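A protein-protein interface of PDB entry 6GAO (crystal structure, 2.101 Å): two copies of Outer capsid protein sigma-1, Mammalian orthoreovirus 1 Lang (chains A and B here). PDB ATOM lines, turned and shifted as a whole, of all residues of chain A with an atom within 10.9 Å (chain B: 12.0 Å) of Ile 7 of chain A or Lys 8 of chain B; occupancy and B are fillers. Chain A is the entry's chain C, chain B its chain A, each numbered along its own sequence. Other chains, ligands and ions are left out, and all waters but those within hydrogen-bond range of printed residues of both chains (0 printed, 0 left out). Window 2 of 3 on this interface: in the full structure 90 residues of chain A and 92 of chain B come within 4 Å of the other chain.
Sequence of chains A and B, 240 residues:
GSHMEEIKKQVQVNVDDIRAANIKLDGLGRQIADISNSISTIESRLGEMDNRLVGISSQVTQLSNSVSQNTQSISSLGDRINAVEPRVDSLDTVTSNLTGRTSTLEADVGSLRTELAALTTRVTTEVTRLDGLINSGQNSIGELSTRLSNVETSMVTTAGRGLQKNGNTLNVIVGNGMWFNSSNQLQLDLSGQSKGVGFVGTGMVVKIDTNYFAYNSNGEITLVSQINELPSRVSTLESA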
ATOM      1  N   MET A   4      12.726   6.899   4.859  1.00  0.00           N
ATOM      2  CA  MET A   4      11.402   6.293   4.773  1.00  0.00           C
ATOM      3  C   MET A   4      11.479   4.807   4.402  1.00  0.00           C
ATOM      4  O   MET A   4      10.683   3.982   4.881  1.00  0.00           O
ATOM      5  CB  MET A   4      10.544   7.032   3.755  1.00  0.00           C
ATOM      6  CG  MET A   4       9.197   6.400   3.515  1.00  0.00           C
ATOM      7  SD  MET A   4       8.277   6.281   5.057  1.00  0.00           S
ATOM      8  N   GLU A   5      12.435   4.468   3.536  1.00  0.00           N
ATOM      9  CA  GLU A   5      12.656   3.066   3.209  1.00  0.00           C
ATOM     10  C   GLU A   5      13.236   2.312   4.400  1.00  0.00           C
ATOM     11  O   GLU A   5      12.894   1.145   4.627  1.00  0.00           O
ATOM     12  CB  GLU A   5      13.581   2.944   1.997  1.00  0.00           C
ATOM     13  CG  GLU A   5      13.339   1.706   1.142  1.00  0.00           C
ATOM     14  CD  GLU A   5      12.217   1.904   0.132  1.00  0.00           C
ATOM     15  OE1 GLU A   5      12.247   2.925  -0.587  1.00  0.00           O
ATOM     16  OE2 GLU A   5      11.308   1.043   0.045  1.00  0.00           O
ATOM     17  N   GLU A   6      14.122   2.954   5.166  1.00  0.00           N
ATOM     18  CA  GLU A   6      14.703   2.282   6.325  1.00  0.00           C
ATOM     19  C   GLU A   6      13.655   2.050   7.408  1.00  0.00           C
ATOM     20  O   GLU A   6      13.794   1.128   8.227  1.00  0.00           O
ATOM     21  CB  GLU A   6      15.882   3.094   6.876  1.00  0.00           C
ATOM     22  N   ILE A   7      12.599   2.865   7.416  1.00  0.00           N
ATOM     23  CA  ILE A   7      11.513   2.658   8.363  1.00  0.00           C
ATOM     24  C   ILE A   7      10.774   1.373   8.029  1.00  0.00           C
ATOM     25  O   ILE A   7      10.523   0.533   8.904  1.00  0.00           O
ATOM     26  CB  ILE A   7      10.578   3.879   8.369  1.00  0.00           C
ATOM     27  CG1 ILE A   7      11.246   5.026   9.119  1.00  0.00           C
ATOM     28  CG2 ILE A   7       9.207   3.534   8.990  1.00  0.00           C
ATOM     29  CD1 ILE A   7      10.328   6.167   9.431  1.00  0.00           C
ATOM     30  N   LYS A   8      10.459   1.184   6.740  1.00  0.00           N
ATOM     31  CA  LYS A   8       9.781  -0.029   6.293  1.00  0.00           C
ATOM     32  C   LYS A   8      10.621  -1.280   6.566  1.00  0.00           C
ATOM     33  O   LYS A   8      10.083  -2.352   6.897  1.00  0.00           O
ATOM     34  CB  LYS A   8       9.447   0.117   4.807  1.00  0.00           C
ATOM     35  CG  LYS A   8       9.023  -1.162   4.097  1.00  0.00           C
ATOM     36  CD  LYS A   8       8.851  -0.934   2.586  1.00  0.00           C
ATOM     37  N   LYS A   9      11.944  -1.162   6.444  1.00  0.00           N
ATOM     38  CA  LYS A   9      12.810  -2.310   6.695  1.00  0.00           C
ATOM     39  C   LYS A   9      12.761  -2.733   8.159  1.00  0.00           C
ATOM     40  O   LYS A   9      12.810  -3.925   8.462  1.00  0.00           O
ATOM     41  CB  LYS A   9      14.243  -1.997   6.287  1.00  0.00           C
ATOM     42  CG  LYS A   9      14.524  -2.337   4.812  1.00  0.00           C
ATOM     43  CD  LYS A   9      15.875  -1.772   4.360  1.00  0.00           C
ATOM     44  N   GLN A  10      12.690  -1.777   9.071  1.00  0.00           N
ATOM     45  CA  GLN A  10      12.617  -2.134  10.475  1.00  0.00           C
ATOM     46  C   GLN A  10      11.237  -2.684  10.812  1.00  0.00           C
ATOM     47  O   GLN A  10      11.123  -3.590  11.637  1.00  0.00           O
ATOM     48  CB  GLN A  10      12.982  -0.932  11.358  1.00  0.00           C
ATOM     49  CG  GLN A  10      12.970  -1.239  12.886  1.00  0.00           C
ATOM     50  CD  GLN A  10      13.988  -2.313  13.243  1.00  0.00           C
ATOM     51  OE1 GLN A  10      15.177  -2.141  12.987  1.00  0.00           O
ATOM     52  NE2 GLN A  10      13.526  -3.437  13.815  1.00  0.00           N
ATOM     53  N   VAL A  11      10.189  -2.180  10.164  1.00  0.00           N
ATOM     54  CA  VAL A  11       8.858  -2.764  10.324  1.00  0.00           C
ATOM     55  C   VAL A  11       8.886  -4.239   9.940  1.00  0.00           C
ATOM     56  O   VAL A  11       8.427  -5.113  10.687  1.00  0.00           O
ATOM     57  CB  VAL A  11       7.824  -1.975   9.493  1.00  0.00           C
ATOM     58  CG1 VAL A  11       6.513  -2.643   9.536  1.00  0.00           C
ATOM     59  CG2 VAL A  11       7.719  -0.554  10.022  1.00  0.00           C
ATOM     60  N   GLN A  12       9.452  -4.537   8.783  1.00  0.00           N
ATOM     61  CA  GLN A  12       9.544  -5.920   8.345  1.00  0.00           C
ATOM     62  C   GLN A  12      10.334  -6.783   9.327  1.00  0.00           C
ATOM     63  O   GLN A  12       9.930  -7.908   9.626  1.00  0.00           O
ATOM     64  CB  GLN A  12      10.155  -5.980   6.949  1.00  0.00           C
ATOM     65  CG  GLN A  12      10.147  -7.426   6.417  1.00  0.00           C
ATOM     66  CD  GLN A  12       8.768  -8.076   6.513  1.00  0.00           C
ATOM     67  OE1 GLN A  12       8.613  -9.174   7.059  1.00  0.00           O
ATOM     68  NE2 GLN A  12       7.750  -7.391   5.970  1.00  0.00           N
ATOM     69  N   VAL A  13      11.449  -6.268   9.854  1.00  0.00           N
ATOM     70  CA  VAL A  13      12.175  -6.971  10.911  1.00  0.00           C
ATOM     71  C   VAL A  13      11.278  -7.198  12.124  1.00  0.00           C
ATOM     72  O   VAL A  13      11.246  -8.300  12.677  1.00  0.00           O
ATOM     73  CB  VAL A  13      13.450  -6.196  11.296  1.00  0.00           C
ATOM     74  CG1 VAL A  13      14.057  -6.776  12.596  1.00  0.00           C
ATOM     75  CG2 VAL A  13      14.459  -6.250  10.146  1.00  0.00           C
ATOM     76  N   ASN A  14      10.508  -6.173  12.539  1.00  0.00           N
ATOM     77  CA  ASN A  14       9.644  -6.344  13.709  1.00  0.00           C
ATOM     78  C   ASN A  14       8.594  -7.418  13.459  1.00  0.00           C
ATOM     79  O   ASN A  14       8.286  -8.214  14.364  1.00  0.00           O
ATOM     80  CB  ASN A  14       8.971  -5.015  14.108  1.00  0.00           C
ATOM     81  CG  ASN A  14       9.940  -4.036  14.745  1.00  0.00           C
ATOM     82  OD1 ASN A  14      11.072  -4.398  15.027  1.00  0.00           O
ATOM     83  ND2 ASN A  14       9.514  -2.783  14.945  1.00  0.00           N
ATOM     84  N   VAL A  15       8.012  -7.450  12.252  1.00  0.00           N
ATOM     85  CA  VAL A  15       7.069  -8.523  11.913  1.00  0.00           C
ATOM     86  C   VAL A  15       7.740  -9.881  12.103  1.00  0.00           C
ATOM     87  O   VAL A  15       7.145 -10.812  12.654  1.00  0.00           O
ATOM     88  CB  VAL A  15       6.548  -8.382  10.468  1.00  0.00           C
ATOM     89  CG1 VAL A  15       5.758  -9.605  10.118  1.00  0.00           C
ATOM     90  CG2 VAL A  15       5.646  -7.104  10.228  1.00  0.00           C
ATOM     91  N   HIS B   3       3.777  13.310  11.037  1.00  0.00           N
ATOM     92  CA  HIS B   3       3.272  12.013  10.588  1.00  0.00           C
ATOM     93  C   HIS B   3       4.417  11.006  10.413  1.00  0.00           C
ATOM     94  O   HIS B   3       4.366   9.901  10.974  1.00  0.00           O
ATOM     95  CB  HIS B   3       2.483  12.150   9.284  1.00  0.00           C
ATOM     96  N   MET B   4       5.451  11.379   9.654  1.00  0.00           N
ATOM     97  CA  MET B   4       6.600  10.487   9.510  1.00  0.00           C
ATOM     98  C   MET B   4       7.313  10.301  10.840  1.00  0.00           C
ATOM     99  O   MET B   4       7.784   9.199  11.160  1.00  0.00           O
ATOM    100  CB  MET B   4       7.589  11.023   8.475  1.00  0.00           C
ATOM    101  CG  MET B   4       8.669  10.018   8.064  1.00  0.00           C
ATOM    102  N   GLU B   5       7.432  11.384  11.609  1.00  0.00           N
ATOM    103  CA  GLU B   5       8.153  11.315  12.864  1.00  0.00           C
ATOM    104  C   GLU B   5       7.372  10.501  13.884  1.00  0.00           C
ATOM    105  O   GLU B   5       7.964   9.773  14.693  1.00  0.00           O
ATOM    106  CB  GLU B   5       8.438  12.733  13.370  1.00  0.00           C
ATOM    107  N   GLU B   6       6.047  10.584  13.831  1.00  0.00           N
ATOM    108  CA  GLU B   6       5.232   9.841  14.769  1.00  0.00           C
ATOM    109  C   GLU B   6       5.326   8.346  14.501  1.00  0.00           C
ATOM    110  O   GLU B   6       5.435   7.551  15.435  1.00  0.00           O
ATOM    111  CB  GLU B   6       3.784  10.328  14.694  1.00  0.00           C
ATOM    112  N   ILE B   7       5.289   7.938  13.231  1.00  0.00           N
ATOM    113  CA  ILE B   7       5.356   6.510  12.940  1.00  0.00           C
ATOM    114  C   ILE B   7       6.744   5.970  13.258  1.00  0.00           C
ATOM    115  O   ILE B   7       6.885   4.862  13.793  1.00  0.00           O
ATOM    116  CB  ILE B   7       4.950   6.230  11.483  1.00  0.00           C
ATOM    117  CG1 ILE B   7       3.420   6.242  11.351  1.00  0.00           C
ATOM    118  CG2 ILE B   7       5.510   4.871  11.013  1.00  0.00           C
ATOM    119  CD1 ILE B   7       2.929   6.187   9.886  1.00  0.00           C
ATOM    120  N   LYS B   8       7.785   6.756  12.965  1.00  0.00           N
ATOM    121  CA  LYS B   8       9.151   6.332  13.256  1.00  0.00           C
ATOM    122  C   LYS B   8       9.353   6.058  14.749  1.00  0.00           C
ATOM    123  O   LYS B   8      10.056   5.108  15.128  1.00  0.00           O
ATOM    124  CB  LYS B   8      10.132   7.386  12.759  1.00  0.00           C
ATOM    125  CG  LYS B   8      11.586   6.966  12.826  1.00  0.00           C
ATOM    126  CD  LYS B   8      12.519   8.169  12.733  1.00  0.00           C
ATOM    127  N   LYS B   9       8.732   6.869  15.614  1.00  0.00           N
ATOM    128  CA  LYS B   9       8.889   6.664  17.048  1.00  0.00           C
ATOM    129  C   LYS B   9       8.148   5.418  17.510  1.00  0.00           C
ATOM    130  O   LYS B   9       8.659   4.670  18.347  1.00  0.00           O
ATOM    131  CB  LYS B   9       8.406   7.896  17.821  1.00  0.00           C
ATOM    132  N   GLN B  10       6.937   5.174  16.988  1.00  0.00           N
ATOM    133  CA  GLN B  10       6.234   3.967  17.390  1.00  0.00           C
ATOM    134  C   GLN B  10       6.972   2.721  16.905  1.00  0.00           C
ATOM    135  O   GLN B  10       6.873   1.673  17.540  1.00  0.00           O
ATOM    136  CB  GLN B  10       4.776   3.978  16.904  1.00  0.00           C
ATOM    137  CG  GLN B  10       3.979   2.737  17.358  1.00  0.00           C
ATOM    138  CD  GLN B  10       3.699   2.713  18.885  1.00  0.00           C
ATOM    139  OE1 GLN B  10       3.024   3.597  19.403  1.00  0.00           O
ATOM    140  NE2 GLN B  10       4.226   1.705  19.598  1.00  0.00           N
ATOM    141  N   VAL B  11       7.758   2.823  15.830  1.00  0.00           N
ATOM    142  CA  VAL B  11       8.526   1.662  15.382  1.00  0.00           C
ATOM    143  C   VAL B  11       9.670   1.373  16.346  1.00  0.00           C
ATOM    144  O   VAL B  11       9.963   0.209  16.645  1.00  0.00           O
ATOM    145  CB  VAL B  11       9.058   1.852  13.956  1.00  0.00           C
ATOM    146  CG1 VAL B  11       9.928   0.662  13.594  1.00  0.00           C
ATOM    147  CG2 VAL B  11       7.935   1.995  12.940  1.00  0.00           C
ATOM    148  N   GLN B  12      10.380   2.416  16.790  1.00  0.00           N
ATOM    149  CA  GLN B  12      11.410   2.211  17.803  1.00  0.00           C
ATOM    150  C   GLN B  12      10.793   1.716  19.108  1.00  0.00           C
ATOM    151  O   GLN B  12      11.394   0.896  19.805  1.00  0.00           O
ATOM    152  CB  GLN B  12      12.192   3.496  18.087  1.00  0.00           C
ATOM    153  CG  GLN B  12      12.904   4.158  16.936  1.00  0.00           C
ATOM    154  CD  GLN B  12      12.992   5.691  17.161  1.00  0.00           C
ATOM    155  OE1 GLN B  12      12.060   6.435  16.831  1.00  0.00           O
ATOM    156  NE2 GLN B  12      14.083   6.146  17.787  1.00  0.00           N
ATOM    157  N   VAL B  13       9.618   2.243  19.482  1.00  0.00           N
ATOM    158  CA  VAL B  13       8.959   1.735  20.687  1.00  0.00           C
ATOM    159  C   VAL B  13       8.677   0.251  20.526  1.00  0.00           C
ATOM    160  O   VAL B  13       8.804  -0.536  21.480  1.00  0.00           O
ATOM    161  CB  VAL B  13       7.665   2.510  20.989  1.00  0.00           C
ATOM    162  CG1 VAL B  13       6.895   1.826  22.161  1.00  0.00           C
ATOM    163  CG2 VAL B  13       7.973   3.998  21.270  1.00  0.00           C
ATOM    164  N   ASN B  14       8.312  -0.157  19.297  1.00  0.00           N
ATOM    165  CA  ASN B  14       8.051  -1.565  19.043  1.00  0.00           C
ATOM    166  C   ASN B  14       9.331  -2.371  19.155  1.00  0.00           C
ATOM    167  O   ASN B  14       9.306  -3.470  19.709  1.00  0.00           O
ATOM    168  CB  ASN B  14       7.388  -1.756  17.667  1.00  0.00           C
ATOM    169  CG  ASN B  14       5.920  -1.389  17.687  1.00  0.00           C
ATOM    170  OD1 ASN B  14       5.344  -1.151  18.762  1.00  0.00           O
ATOM    171  ND2 ASN B  14       5.289  -1.365  16.511  1.00  0.00           N
ATOM    172  N   VAL B  15      10.460  -1.831  18.666  1.00  0.00           N
ATOM    173  CA  VAL B  15      11.725  -2.561  18.794  1.00  0.00           C
ATOM    174  C   VAL B  15      12.012  -2.857  20.255  1.00  0.00           C
ATOM    175  O   VAL B  15      12.397  -3.983  20.605  1.00  0.00           O
ATOM    176  CB  VAL B  15      12.901  -1.802  18.140  1.00  0.00           C
ATOM    177  CG1 VAL B  15      14.239  -2.506  18.469  1.00  0.00           C
ATOM    178  CG2 VAL B  15      12.728  -1.712  16.622  1.00  0.00           C
ATOM    179  N   ASP B  16      11.786  -1.862  21.137  1.00  0.00           N
ATOM    180  CA  ASP B  16      12.093  -2.026  22.558  1.00  0.00           C
ATOM    181  C   ASP B  16      11.083  -2.929  23.251  1.00  0.00           C
ATOM    182  O   ASP B  16      11.448  -3.683  24.154  1.00  0.00           O
ATOM    183  CB  ASP B  16      12.140  -0.663  23.268  1.00  0.00           C
ATOM    184  CG  ASP B  16      13.206   0.280  22.700  1.00  0.00           C
ATOM    185  OD1 ASP B  16      14.222  -0.200  22.139  1.00  0.00           O
ATOM    186  OD2 ASP B  16      13.032   1.515  22.833  1.00  0.00           O
ATOM    187  N   ASP B  17       9.820  -2.900  22.835  1.00  0.00           N
ATOM    188  CA  ASP B  17       8.857  -3.798  23.464  1.00  0.00           C
ATOM    189  C   ASP B  17       9.085  -5.239  23.064  1.00  0.00           C
ATOM    190  O   ASP B  17       8.852  -6.158  23.865  1.00  0.00           O
ATOM    191  CB  ASP B  17       7.440  -3.381  23.116  1.00  0.00           C
ATOM    192  CG  ASP B  17       7.113  -2.024  23.686  1.00  0.00           C
ATOM    193  OD1 ASP B  17       7.919  -1.555  24.532  1.00  0.00           O
ATOM    194  OD2 ASP B  17       6.089  -1.429  23.274  1.00  0.00           O
ATOM    195  N   ILE B  18       9.431  -5.464  21.798  1.00  0.00           N
ATOM    196  CA  ILE B  18       9.757  -6.808  21.369  1.00  0.00           C
ATOM    197  C   ILE B  18      10.901  -7.331  22.203  1.00  0.00           C
ATOM    198  O   ILE B  18      10.837  -8.430  22.751  1.00  0.00           O
ATOM    199  CB  ILE B  18      10.097  -6.837  19.866  1.00  0.00           C
ATOM    200  CG1 ILE B  18       8.858  -6.471  19.047  1.00  0.00           C
ATOM    201  CG2 ILE B  18      10.552  -8.238  19.521  1.00  0.00           C
ATOM    202  CD1 ILE B  18       9.089  -6.115  17.560  1.00  0.00           C
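Ile 7 of chain A touches Lys 8 of chain B, but with the chains exchanged Lys 8 of chain A does not touch Ile 7 of chain B (7.5 Å).
Gln 10 of chain A touches Val 11 of chain B, but with the chains exchanged Val 11 of chain A does not touch Gln 10 of chain B (7.7 Å).
Gln 10 of chain A touches Val 15 of chain B, but with the chains exchanged Val 15 of chain A does not touch Gln 10 of chain B (10.6 Å).
Asn 14 of chain A touches Val 11 of chain B, but with the chains exchanged Val 11 of chain A does not touch Asn 14 of chain B (7.0 Å).
Of the 8 pairs that touch across the chains among the printed residues, 2 have their exchanged pair printed and touching as well.
Of the 16 printed residues of chain B, 5 touch a printed residue of chain A.
Hydrophobic or aromatic side chains of chain B within 4 Å of the printed part of chain A: Val 11, Val 15 and Ile 18.
Of the 12 printed residues of chain A, 4 touch a printed residue of chain B.
Printed residues of chain A that touch a printed residue of chain B: Ile 7, Gln 10, Val 11 and Asn 14.
Hydrophobic or aromatic side chains of chain A that line the printed part of chain B: Ile 7 and Val 11.
Among the printed residues, no Asp or Glu carboxylate lies within 4 Å of a Lys or Arg side-chain nitrogen of the other chain.
Of chain B, only Lys 8 (3.5 Å) comes within 4 Å of Ile 7 of chain A.
No residue of chain B comes within 4 Å of Met 4 of chain A.
No residue of chain B comes within 4 Å of Lys 8 of chain A.
No residue of chain B comes within 4 Å of Lys 9 of chain A.
Printed residues of chain B within 4 Å of Gln 10 of chain A: Val 11 (3.7 Å) and Val 15 (3.4 Å).
Of chain B, only Val 11 comes within 4 Å of Val 11 of chain A.
Glu 5 of chain B touches none of the printed residues of chain A.
No residue of chain A comes within 4 Å of Glu 6 of chain B.
No residue of chain A comes within 4 Å of Lys 9 of chain B.
Of chain A, only Gln 10 (3.7 Å), Val 11 (3.9 Å) and Asn 14 (3.5 Å) come within 4 Å of Val 11 of chain B.
Of the printed residues of chain A, Ile 18 of chain B touches Asn 14 (3.6 Å).
Of the printed residues of chain A, Val 15 of chain B touches Gln 10 (3.4 Å) and Asn 14 (3.5 Å).
Val 15 of chain A touches none of the printed residues of chain B.
Glu 5 of chain A touches none of the printed residues of chain B.
The nearest printed residue of chain A that does not touch Asn 14 of chain B is Gln 10 of chain A (6.9 Å).
OD1 of Asn 14 of chain A is in hydrogen-bond range of NE2 of Gln 10 of chain A (2.9 Å).
The backbone carbonyl oxygen (O) of Lys 8 of chain B sits close to the side-chain amide oxygen (OE1) of Gln 12 of chain B (2.9 Å).
The side-chain amide nitrogen of Gln 10 of chain B lies within hydrogen-bond range of the side-chain amide oxygen of Asn 14 of chain B.
Among the printed residues, pairs that only touch across the chains: Ile 7 of chain A with Lys 8 of chain B, Gln 10 of chain A with Val 11 of chain B, Gln 10 of chain A with Val 15 of chain B, Val 11 of chain A with Val 11 of chain B, Asn 14 of chain A with Asn 14 of chain B, Asn 14 of chain A with Val 15 of chain B and Asn 14 of chain A with Ile 18 of chain B.
ND2 of Asn 14 of chain A sits at hydrogen-bond distance from O of Val 11 of chain B (3.5 Å).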
